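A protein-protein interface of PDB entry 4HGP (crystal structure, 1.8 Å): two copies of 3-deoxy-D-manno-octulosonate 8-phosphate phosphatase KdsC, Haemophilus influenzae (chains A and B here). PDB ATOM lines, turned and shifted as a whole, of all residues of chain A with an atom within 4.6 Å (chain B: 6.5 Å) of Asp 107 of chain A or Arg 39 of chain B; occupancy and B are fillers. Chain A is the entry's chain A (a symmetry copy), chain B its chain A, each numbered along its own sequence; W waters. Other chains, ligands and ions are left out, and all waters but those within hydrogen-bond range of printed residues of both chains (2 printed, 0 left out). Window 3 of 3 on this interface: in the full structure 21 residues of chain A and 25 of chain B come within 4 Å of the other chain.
Water W2 lies within hydrogen-bond range of OD2 of Asp 126 of chain A, NH1 of Arg 39 of chain B and O of Gly 17 of chain A. Water W1 bridges the side-chain carboxylate of Asp 108 of chain A (2.9 Å) and the guanidinium group of Arg 149 of chain B (3.3 Å).
Asp 107 of chain A touches just one residue of chain B: Arg 39. Of chain A, only Asp 107 (2.9 Å), Asp 108 (3.6 Å) and Asp 126 (3.3 Å) come within 4 Å of Arg 39 of chain B. Of the printed residues of chain A, Leu 42 of chain B touches Asp 108 (3.4 Å). Of the printed residues of chain A, Val 38 of chain B touches Asp 16. Printed residues of chain B within 4 Å of Asp 16 of chain A: Val 38. The nearest residue of chain B that does not touch Asp 107 of chain A is Val 38 of chain B (4.8 Å).
The backbone NH (N) of Asp 107 of chain A lies within hydrogen-bond range of the side-chain carboxylate (OD2) of Asp 111 of chain A, 2.8 Å away. NH1 of Arg 149 of chain B is in hydrogen-bond range of O of Arg 39 of chain B (3.1 Å). The side-chain carboxylate (OD2) of Asp 111 of chain A lies within hydrogen-bond range of the backbone NH (N) of Asp 108 of chain A (3.0 Å). NE2 of His 37 of chain B sits close to NH2 of Arg 39 of chain B. OD1 of Asp 40 of chain B lies within hydrogen-bond range of N of Arg 149 of chain B, 3.0 Å away. O of Arg 149 of chain B lies within hydrogen-bond range of OG of Ser 152 of chain B.
Among the printed residues, pairs that only touch across the chains: Asp 16 of chain A with Val 38 of chain B (3.9 Å), Asp 108 of chain A with Arg 39 of chain B (3.6 Å) and Asp 108 of chain A with Leu 42 of chain B (3.4 Å).
Of the 14 printed residues of chain B, 4 touch a printed residue of chain A. Printed residues of chain B that touch a printed residue of chain A: Val 38, Arg 39, Leu 42 and Arg 149. Of the 13 printed residues of chain A, 4 touch a printed residue of chain B. Along chain A the printed residues that touch a printed residue of chain B span positions 16 to 126. Among the printed residues, Asp or Glu carboxylates within 4 Å of a Lys or Arg side-chain nitrogen of the other chain: Asp 107 of chain A with Arg 39 of chain B, Asp 108 of chain A with Arg 149 of chain B and Asp 126 of chain A with Arg 39 of chain B.
OD2 of Asp 108 of chain A is in salt-bridge range of NH1 of Arg 149 of chain B (2.8 Å). The side-chain carboxylate (OD2) of Asp 107 of chain A lies within salt-bridge range of the guanidinium group (NH1) of Arg 39 of chain B, 2.9 Å away. The guanidinium group (NH2) of Arg 39 of chain B is in salt-bridge range of the side-chain carboxylate (OD2) of Asp 126 of chain A, at 3.3 Å.
No position is printed for both chains. Of the 6 pairs that touch across the chains among the printed residues, none has its exchanged pair printed and touching as well.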
ATOM      1  N   ASP A  14      32.440  23.249   1.297  1.00  0.00           N
ATOM      2  CA  ASP A  14      32.087  24.386   0.475  1.00  0.00           C
ATOM      3  C   ASP A  14      30.779  24.982   1.018  1.00  0.00           C
ATOM      4  O   ASP A  14      30.057  24.315   1.751  1.00  0.00           O
ATOM      5  CB  ASP A  14      31.899  23.912  -0.955  1.00  0.00           C
ATOM      6  CG  ASP A  14      31.363  24.984  -1.837  1.00  0.00           C
ATOM      7  OD1 ASP A  14      31.940  26.087  -1.806  1.00  0.00           O
ATOM      8  OD2 ASP A  14      30.349  24.738  -2.518  1.00  0.00           O
ATOM      9  N   ASP A  16      28.293  27.619  -0.862  1.00  0.00           N
ATOM     10  CA  ASP A  16      27.187  27.830  -1.784  1.00  0.00           C
ATOM     11  C   ASP A  16      26.885  26.535  -2.517  1.00  0.00           C
ATOM     12  O   ASP A  16      27.765  25.958  -3.177  1.00  0.00           O
ATOM     13  CB  ASP A  16      27.486  28.970  -2.767  1.00  0.00           C
ATOM     14  CG  ASP A  16      27.894  30.256  -2.069  1.00  0.00           C
ATOM     15  OD1 ASP A  16      27.056  30.822  -1.332  1.00  0.00           O
ATOM     16  OD2 ASP A  16      29.050  30.706  -2.257  1.00  0.00           O
ATOM     17  N   GLY A  17      25.647  26.070  -2.371  1.00  0.00           N
ATOM     18  CA  GLY A  17      25.202  24.847  -3.016  1.00  0.00           C
ATOM     19  C   GLY A  17      25.493  23.593  -2.208  1.00  0.00           C
ATOM     20  O   GLY A  17      25.200  22.476  -2.643  1.00  0.00           O
ATOM     21  N   VAL A  18      26.067  23.774  -1.026  1.00  0.00           N
ATOM     22  CA  VAL A  18      26.289  22.662  -0.108  1.00  0.00           C
ATOM     23  C   VAL A  18      25.622  22.958   1.229  1.00  0.00           C
ATOM     24  O   VAL A  18      24.702  22.246   1.640  1.00  0.00           O
ATOM     25  CB  VAL A  18      27.787  22.356   0.087  1.00  0.00           C
ATOM     26  CG1 VAL A  18      28.003  21.455   1.313  1.00  0.00           C
ATOM     27  CG2 VAL A  18      28.337  21.689  -1.167  1.00  0.00           C
ATOM     28  N   GLY A 106      31.445  19.069  -1.813  1.00  0.00           N
ATOM     29  CA  GLY A 106      31.274  20.158  -2.767  1.00  0.00           C
ATOM     30  C   GLY A 106      30.096  19.953  -3.705  1.00  0.00           C
ATOM     31  O   GLY A 106      29.371  18.976  -3.570  1.00  0.00           O
ATOM     32  N   ASP A 107      29.900  20.862  -4.659  1.00  0.00           N
ATOM     33  CA  ASP A 107      28.792  20.735  -5.608  1.00  0.00           C
ATOM     34  C   ASP A 107      29.083  21.167  -7.041  1.00  0.00           C
ATOM     35  O   ASP A 107      28.223  21.012  -7.906  1.00  0.00           O
ATOM     36  CB  ASP A 107      27.593  21.557  -5.132  1.00  0.00           C
ATOM     37  CG  ASP A 107      27.775  23.043  -5.393  1.00  0.00           C
ATOM     38  OD1 ASP A 107      28.540  23.670  -4.640  1.00  0.00           O
ATOM     39  OD2 ASP A 107      27.168  23.587  -6.345  1.00  0.00           O
ATOM     40  N   ASP A 108      30.251  21.742  -7.302  1.00  0.00           N
ATOM     41  CA  ASP A 108      30.505  22.311  -8.621  1.00  0.00           C
ATOM     42  C   ASP A 108      31.977  22.199  -9.019  1.00  0.00           C
ATOM     43  O   ASP A 108      32.812  21.756  -8.233  1.00  0.00           O
ATOM     44  CB  ASP A 108      30.009  23.766  -8.683  1.00  0.00           C
ATOM     45  CG  ASP A 108      29.733  24.247 -10.108  1.00  0.00           C
ATOM     46  OD1 ASP A 108      29.671  23.412 -11.038  1.00  0.00           O
ATOM     47  OD2 ASP A 108      29.559  25.473 -10.290  1.00  0.00           O
ATOM     48  N   ASP A 111      35.142  22.844  -6.995  1.00  0.00           N
ATOM     49  CA  ASP A 111      35.439  21.883  -5.948  1.00  0.00           C
ATOM     50  C   ASP A 111      36.278  20.721  -6.458  1.00  0.00           C
ATOM     51  O   ASP A 111      36.823  19.961  -5.667  1.00  0.00           O
ATOM     52  CB  ASP A 111      34.135  21.352  -5.367  1.00  0.00           C
ATOM     53  CG  ASP A 111      33.305  22.442  -4.713  1.00  0.00           C
ATOM     54  OD1 ASP A 111      33.843  23.150  -3.842  1.00  0.00           O
ATOM     55  OD2 ASP A 111      32.117  22.588  -5.069  1.00  0.00           O
ATOM     56  N   VAL A 124      26.886  16.675  -3.226  1.00  0.00           N
ATOM     57  CA  VAL A 124      25.469  16.821  -2.901  1.00  0.00           C
ATOM     58  C   VAL A 124      24.632  16.217  -4.022  1.00  0.00           C
ATOM     59  O   VAL A 124      25.119  16.041  -5.130  1.00  0.00           O
ATOM     60  CB  VAL A 124      25.066  18.295  -2.692  1.00  0.00           C
ATOM     61  CG1 VAL A 124      25.805  18.901  -1.485  1.00  0.00           C
ATOM     62  CG2 VAL A 124      25.297  19.096  -3.956  1.00  0.00           C
ATOM     63  N   ASP A 126      22.216  17.249  -5.933  1.00  0.00           N
ATOM     64  CA  ASP A 126      21.908  18.058  -7.113  1.00  0.00           C
ATOM     65  C   ASP A 126      23.157  18.531  -7.878  1.00  0.00           C
ATOM     66  O   ASP A 126      23.071  19.381  -8.771  1.00  0.00           O
ATOM     67  CB  ASP A 126      20.979  19.233  -6.765  1.00  0.00           C
ATOM     68  CG  ASP A 126      21.451  20.041  -5.565  1.00  0.00           C
ATOM     69  OD1 ASP A 126      21.967  19.462  -4.591  1.00  0.00           O
ATOM     70  OD2 ASP A 126      21.295  21.274  -5.597  1.00  0.00           O
ATOM     71  N   ALA A 127      24.304  17.961  -7.526  1.00  0.00           N
ATOM     72  CA  ALA A 127      25.554  18.226  -8.227  1.00  0.00           C
ATOM     73  C   ALA A 127      25.499  17.697  -9.654  1.00  0.00           C
ATOM     74  O   ALA A 127      24.828  16.703  -9.918  1.00  0.00           O
ATOM     75  CB  ALA A 127      26.737  17.591  -7.472  1.00  0.00           C
ATOM     76  N   PRO A 128      26.234  18.347 -10.578  1.00  0.00           N
ATOM     77  CA  PRO A 128      26.232  17.915 -11.982  1.00  0.00           C
ATOM     78  C   PRO A 128      26.968  16.595 -12.133  1.00  0.00           C
ATOM     79  O   PRO A 128      27.706  16.216 -11.229  1.00  0.00           O
ATOM     80  CB  PRO A 128      27.001  19.027 -12.694  1.00  0.00           C
ATOM     81  CG  PRO A 128      27.884  19.583 -11.665  1.00  0.00           C
ATOM     82  CD  PRO A 128      27.169  19.463 -10.354  1.00  0.00           C
ATOM     83  N   VAL A 131      30.701  16.308 -11.522  1.00  0.00           N
ATOM     84  CA  VAL A 131      31.099  16.429 -10.126  1.00  0.00           C
ATOM     85  C   VAL A 131      30.858  15.109  -9.403  1.00  0.00           C
ATOM     86  O   VAL A 131      31.712  14.652  -8.640  1.00  0.00           O
ATOM     87  CB  VAL A 131      30.362  17.587  -9.431  1.00  0.00           C
ATOM     88  CG1 VAL A 131      30.486  17.476  -7.926  1.00  0.00           C
ATOM     89  CG2 VAL A 131      30.921  18.915  -9.929  1.00  0.00           C
ATOM     90  N   HIS B  37      21.304  32.073  -8.933  1.00  0.00           N
ATOM     91  CA  HIS B  37      21.888  30.781  -8.588  1.00  0.00           C
ATOM     92  C   HIS B  37      23.406  30.746  -8.810  1.00  0.00           C
ATOM     93  O   HIS B  37      23.905  31.195  -9.839  1.00  0.00           O
ATOM     94  CB  HIS B  37      21.174  29.666  -9.347  1.00  0.00           C
ATOM     95  CG  HIS B  37      21.520  28.303  -8.849  1.00  0.00           C
ATOM     96  ND1 HIS B  37      20.692  27.583  -8.016  1.00  0.00           N
ATOM     97  CD2 HIS B  37      22.626  27.547  -9.026  1.00  0.00           C
ATOM     98  CE1 HIS B  37      21.265  26.433  -7.718  1.00  0.00           C
ATOM     99  NE2 HIS B  37      22.443  26.388  -8.313  1.00  0.00           N
ATOM    100  N   VAL B  38      24.143  30.222  -7.835  1.00  0.00           N
ATOM    101  CA  VAL B  38      25.608  30.242  -7.888  1.00  0.00           C
ATOM    102  C   VAL B  38      26.232  29.470  -9.059  1.00  0.00           C
ATOM    103  O   VAL B  38      27.218  29.924  -9.643  1.00  0.00           O
ATOM    104  CB  VAL B  38      26.238  29.794  -6.540  1.00  0.00           C
ATOM    105  CG1 VAL B  38      26.120  28.294  -6.346  1.00  0.00           C
ATOM    106  CG2 VAL B  38      27.666  30.202  -6.476  1.00  0.00           C
ATOM    107  N   ARG B  39      25.647  28.325  -9.417  1.00  0.00           N
ATOM    108  CA  ARG B  39      26.157  27.523 -10.521  1.00  0.00           C
ATOM    109  C   ARG B  39      25.823  28.185 -11.848  1.00  0.00           C
ATOM    110  O   ARG B  39      26.507  27.980 -12.848  1.00  0.00           O
ATOM    111  CB  ARG B  39      25.637  26.084 -10.452  1.00  0.00           C
ATOM    112  CG  ARG B  39      26.090  25.346  -9.200  1.00  0.00           C
ATOM    113  CD  ARG B  39      25.848  23.851  -9.293  1.00  0.00           C
ATOM    114  NE  ARG B  39      24.427  23.506  -9.242  1.00  0.00           N
ATOM    115  CZ  ARG B  39      23.766  23.216  -8.126  1.00  0.00           C
ATOM    116  NH1 ARG B  39      24.388  23.246  -6.955  1.00  0.00           N
ATOM    117  NH2 ARG B  39      22.473  22.917  -8.177  1.00  0.00           N
ATOM    118  N   ASP B  40      24.777  29.007 -11.857  1.00  0.00           N
ATOM    119  CA  ASP B  40      24.506  29.840 -13.027  1.00  0.00           C
ATOM    120  C   ASP B  40      25.631  30.853 -13.213  1.00  0.00           C
ATOM    121  O   ASP B  40      26.135  31.049 -14.327  1.00  0.00           O
ATOM    122  CB  ASP B  40      23.157  30.560 -12.908  1.00  0.00           C
ATOM    123  CG  ASP B  40      21.978  29.641 -13.143  1.00  0.00           C
ATOM    124  OD1 ASP B  40      22.167  28.547 -13.713  1.00  0.00           O
ATOM    125  OD2 ASP B  40      20.846  30.017 -12.768  1.00  0.00           O
ATOM    126  N   GLY B  41      26.038  31.479 -12.109  1.00  0.00           N
ATOM    127  CA  GLY B  41      27.046  32.521 -12.152  1.00  0.00           C
ATOM    128  C   GLY B  41      28.348  32.002 -12.721  1.00  0.00           C
ATOM    129  O   GLY B  41      28.988  32.663 -13.534  1.00  0.00           O
ATOM    130  N   LEU B  42      28.736  30.805 -12.291  1.00  0.00           N
ATOM    131  CA  LEU B  42      29.955  30.197 -12.786  1.00  0.00           C
ATOM    132  C   LEU B  42      29.839  29.884 -14.266  1.00  0.00           C
ATOM    133  O   LEU B  42      30.808  30.015 -14.986  1.00  0.00           O
ATOM    134  CB  LEU B  42      30.321  28.939 -12.006  1.00  0.00           C
ATOM    135  CG  LEU B  42      31.798  28.583 -12.198  1.00  0.00           C
ATOM    136  CD1 LEU B  42      32.691  29.776 -11.896  1.00  0.00           C
ATOM    137  CD2 LEU B  42      32.175  27.394 -11.330  1.00  0.00           C
ATOM    138  N   GLY B  43      28.651  29.477 -14.709  1.00  0.00           N
ATOM    139  CA  GLY B  43      28.415  29.197 -16.113  1.00  0.00           C
ATOM    140  C   GLY B  43      28.562  30.453 -16.948  1.00  0.00           C
ATOM    141  O   GLY B  43      29.089  30.417 -18.067  1.00  0.00           O
ATOM    142  N   ILE B  44      28.100  31.572 -16.399  1.00  0.00           N
ATOM    143  CA  ILE B  44      28.205  32.872 -17.066  1.00  0.00           C
ATOM    144  C   ILE B  44      29.663  33.254 -17.293  1.00  0.00           C
ATOM    145  O   ILE B  44      30.032  33.697 -18.382  1.00  0.00           O
ATOM    146  CB  ILE B  44      27.458  33.982 -16.274  1.00  0.00           C
ATOM    147  CG1 ILE B  44      25.954  33.896 -16.544  1.00  0.00           C
ATOM    148  CG2 ILE B  44      27.978  35.367 -16.651  1.00  0.00           C
ATOM    149  CD1 ILE B  44      25.102  34.724 -15.606  1.00  0.00           C
ATOM    150  N   ARG B  68      23.985  42.562  -9.448  1.00  0.00           N
ATOM    151  CA  ARG B  68      24.342  41.204  -9.864  1.00  0.00           C
ATOM    152  C   ARG B  68      25.009  41.218 -11.241  1.00  0.00           C
ATOM    153  O   ARG B  68      25.985  40.502 -11.492  1.00  0.00           O
ATOM    154  CB  ARG B  68      23.105  40.305  -9.875  1.00  0.00           C
ATOM    155  CG  ARG B  68      23.374  38.874 -10.318  1.00  0.00           C
ATOM    156  CD  ARG B  68      24.324  38.145  -9.378  1.00  0.00           C
ATOM    157  NE  ARG B  68      24.382  36.710  -9.675  1.00  0.00           N
ATOM    158  CZ  ARG B  68      25.369  35.901  -9.301  1.00  0.00           C
ATOM    159  NH1 ARG B  68      26.390  36.378  -8.606  1.00  0.00           N
ATOM    160  NH2 ARG B  68      25.337  34.616  -9.628  1.00  0.00           N
ATOM    161  N   LYS B 145      17.365  27.299 -10.857  1.00  0.00           N
ATOM    162  CA  LYS B 145      17.946  26.112 -10.243  1.00  0.00           C
ATOM    163  C   LYS B 145      19.149  25.574 -11.022  1.00  0.00           C
ATOM    164  O   LYS B 145      19.598  24.462 -10.784  1.00  0.00           O
ATOM    165  CB  LYS B 145      16.879  25.028 -10.096  1.00  0.00           C
ATOM    166  CG  LYS B 145      15.632  25.454  -9.314  1.00  0.00           C
ATOM    167  CD  LYS B 145      15.950  25.775  -7.860  1.00  0.00           C
ATOM    168  CE  LYS B 145      14.702  26.245  -7.124  1.00  0.00           C
ATOM    169  NZ  LYS B 145      15.026  26.999  -5.877  1.00  0.00           N
ATOM    170  N   GLY B 146      19.671  26.360 -11.957  1.00  0.00           N
ATOM    171  CA  GLY B 146      20.810  25.922 -12.735  1.00  0.00           C
ATOM    172  C   GLY B 146      20.462  25.731 -14.198  1.00  0.00           C
ATOM    173  O   GLY B 146      21.211  25.099 -14.941  1.00  0.00           O
ATOM    174  N   PHE B 148      20.340  27.984 -16.525  1.00  0.00           N
ATOM    175  CA  PHE B 148      21.329  28.662 -17.357  1.00  0.00           C
ATOM    176  C   PHE B 148      22.592  27.800 -17.461  1.00  0.00           C
ATOM    177  O   PHE B 148      23.089  27.562 -18.553  1.00  0.00           O
ATOM    178  CB  PHE B 148      21.662  30.055 -16.817  1.00  0.00           C
ATOM    179  CG  PHE B 148      22.575  30.849 -17.711  1.00  0.00           C
ATOM    180  CD1 PHE B 148      23.947  30.643 -17.690  1.00  0.00           C
ATOM    181  CD2 PHE B 148      22.060  31.815 -18.560  1.00  0.00           C
ATOM    182  CE1 PHE B 148      24.790  31.369 -18.518  1.00  0.00           C
ATOM    183  CE2 PHE B 148      22.900  32.549 -19.390  1.00  0.00           C
ATOM    184  CZ  PHE B 148      24.266  32.328 -19.365  1.00  0.00           C
ATOM    185  N   ARG B 149      23.085  27.309 -16.325  1.00  0.00           N
ATOM    186  CA  ARG B 149      24.298  26.484 -16.322  1.00  0.00           C
ATOM    187  C   ARG B 149      24.158  25.224 -17.185  1.00  0.00           C
ATOM    188  O   ARG B 149      25.122  24.779 -17.807  1.00  0.00           O
ATOM    189  CB  ARG B 149      24.681  26.093 -14.892  1.00  0.00           C
ATOM    190  CG  ARG B 149      25.907  25.191 -14.789  1.00  0.00           C
ATOM    191  CD  ARG B 149      27.167  25.809 -15.385  1.00  0.00           C
ATOM    192  NE  ARG B 149      28.334  24.977 -15.106  1.00  0.00           N
ATOM    193  CZ  ARG B 149      28.987  24.966 -13.947  1.00  0.00           C
ATOM    194  NH1 ARG B 149      28.599  25.759 -12.951  1.00  0.00           N
ATOM    195  NH2 ARG B 149      30.031  24.162 -13.780  1.00  0.00           N
ATOM    196  N   SER B 152      24.620  26.585 -20.637  1.00  0.00           N
ATOM    197  CA  SER B 152      26.022  26.959 -20.836  1.00  0.00           C
ATOM    198  C   SER B 152      26.925  25.731 -20.942  1.00  0.00           C
ATOM    199  O   SER B 152      27.874  25.723 -21.721  1.00  0.00           O
ATOM    200  CB  SER B 152      26.526  27.927 -19.757  1.00  0.00           C
ATOM    201  OG  SER B 152      26.591  27.339 -18.464  1.00  0.00           O
HETATM  202  O   HOH W   1      27.321  22.728 -12.526  1.00  0.00           O
HETATM  203  O   HOH W   2      22.878  22.818  -4.589  1.00  0.00           O
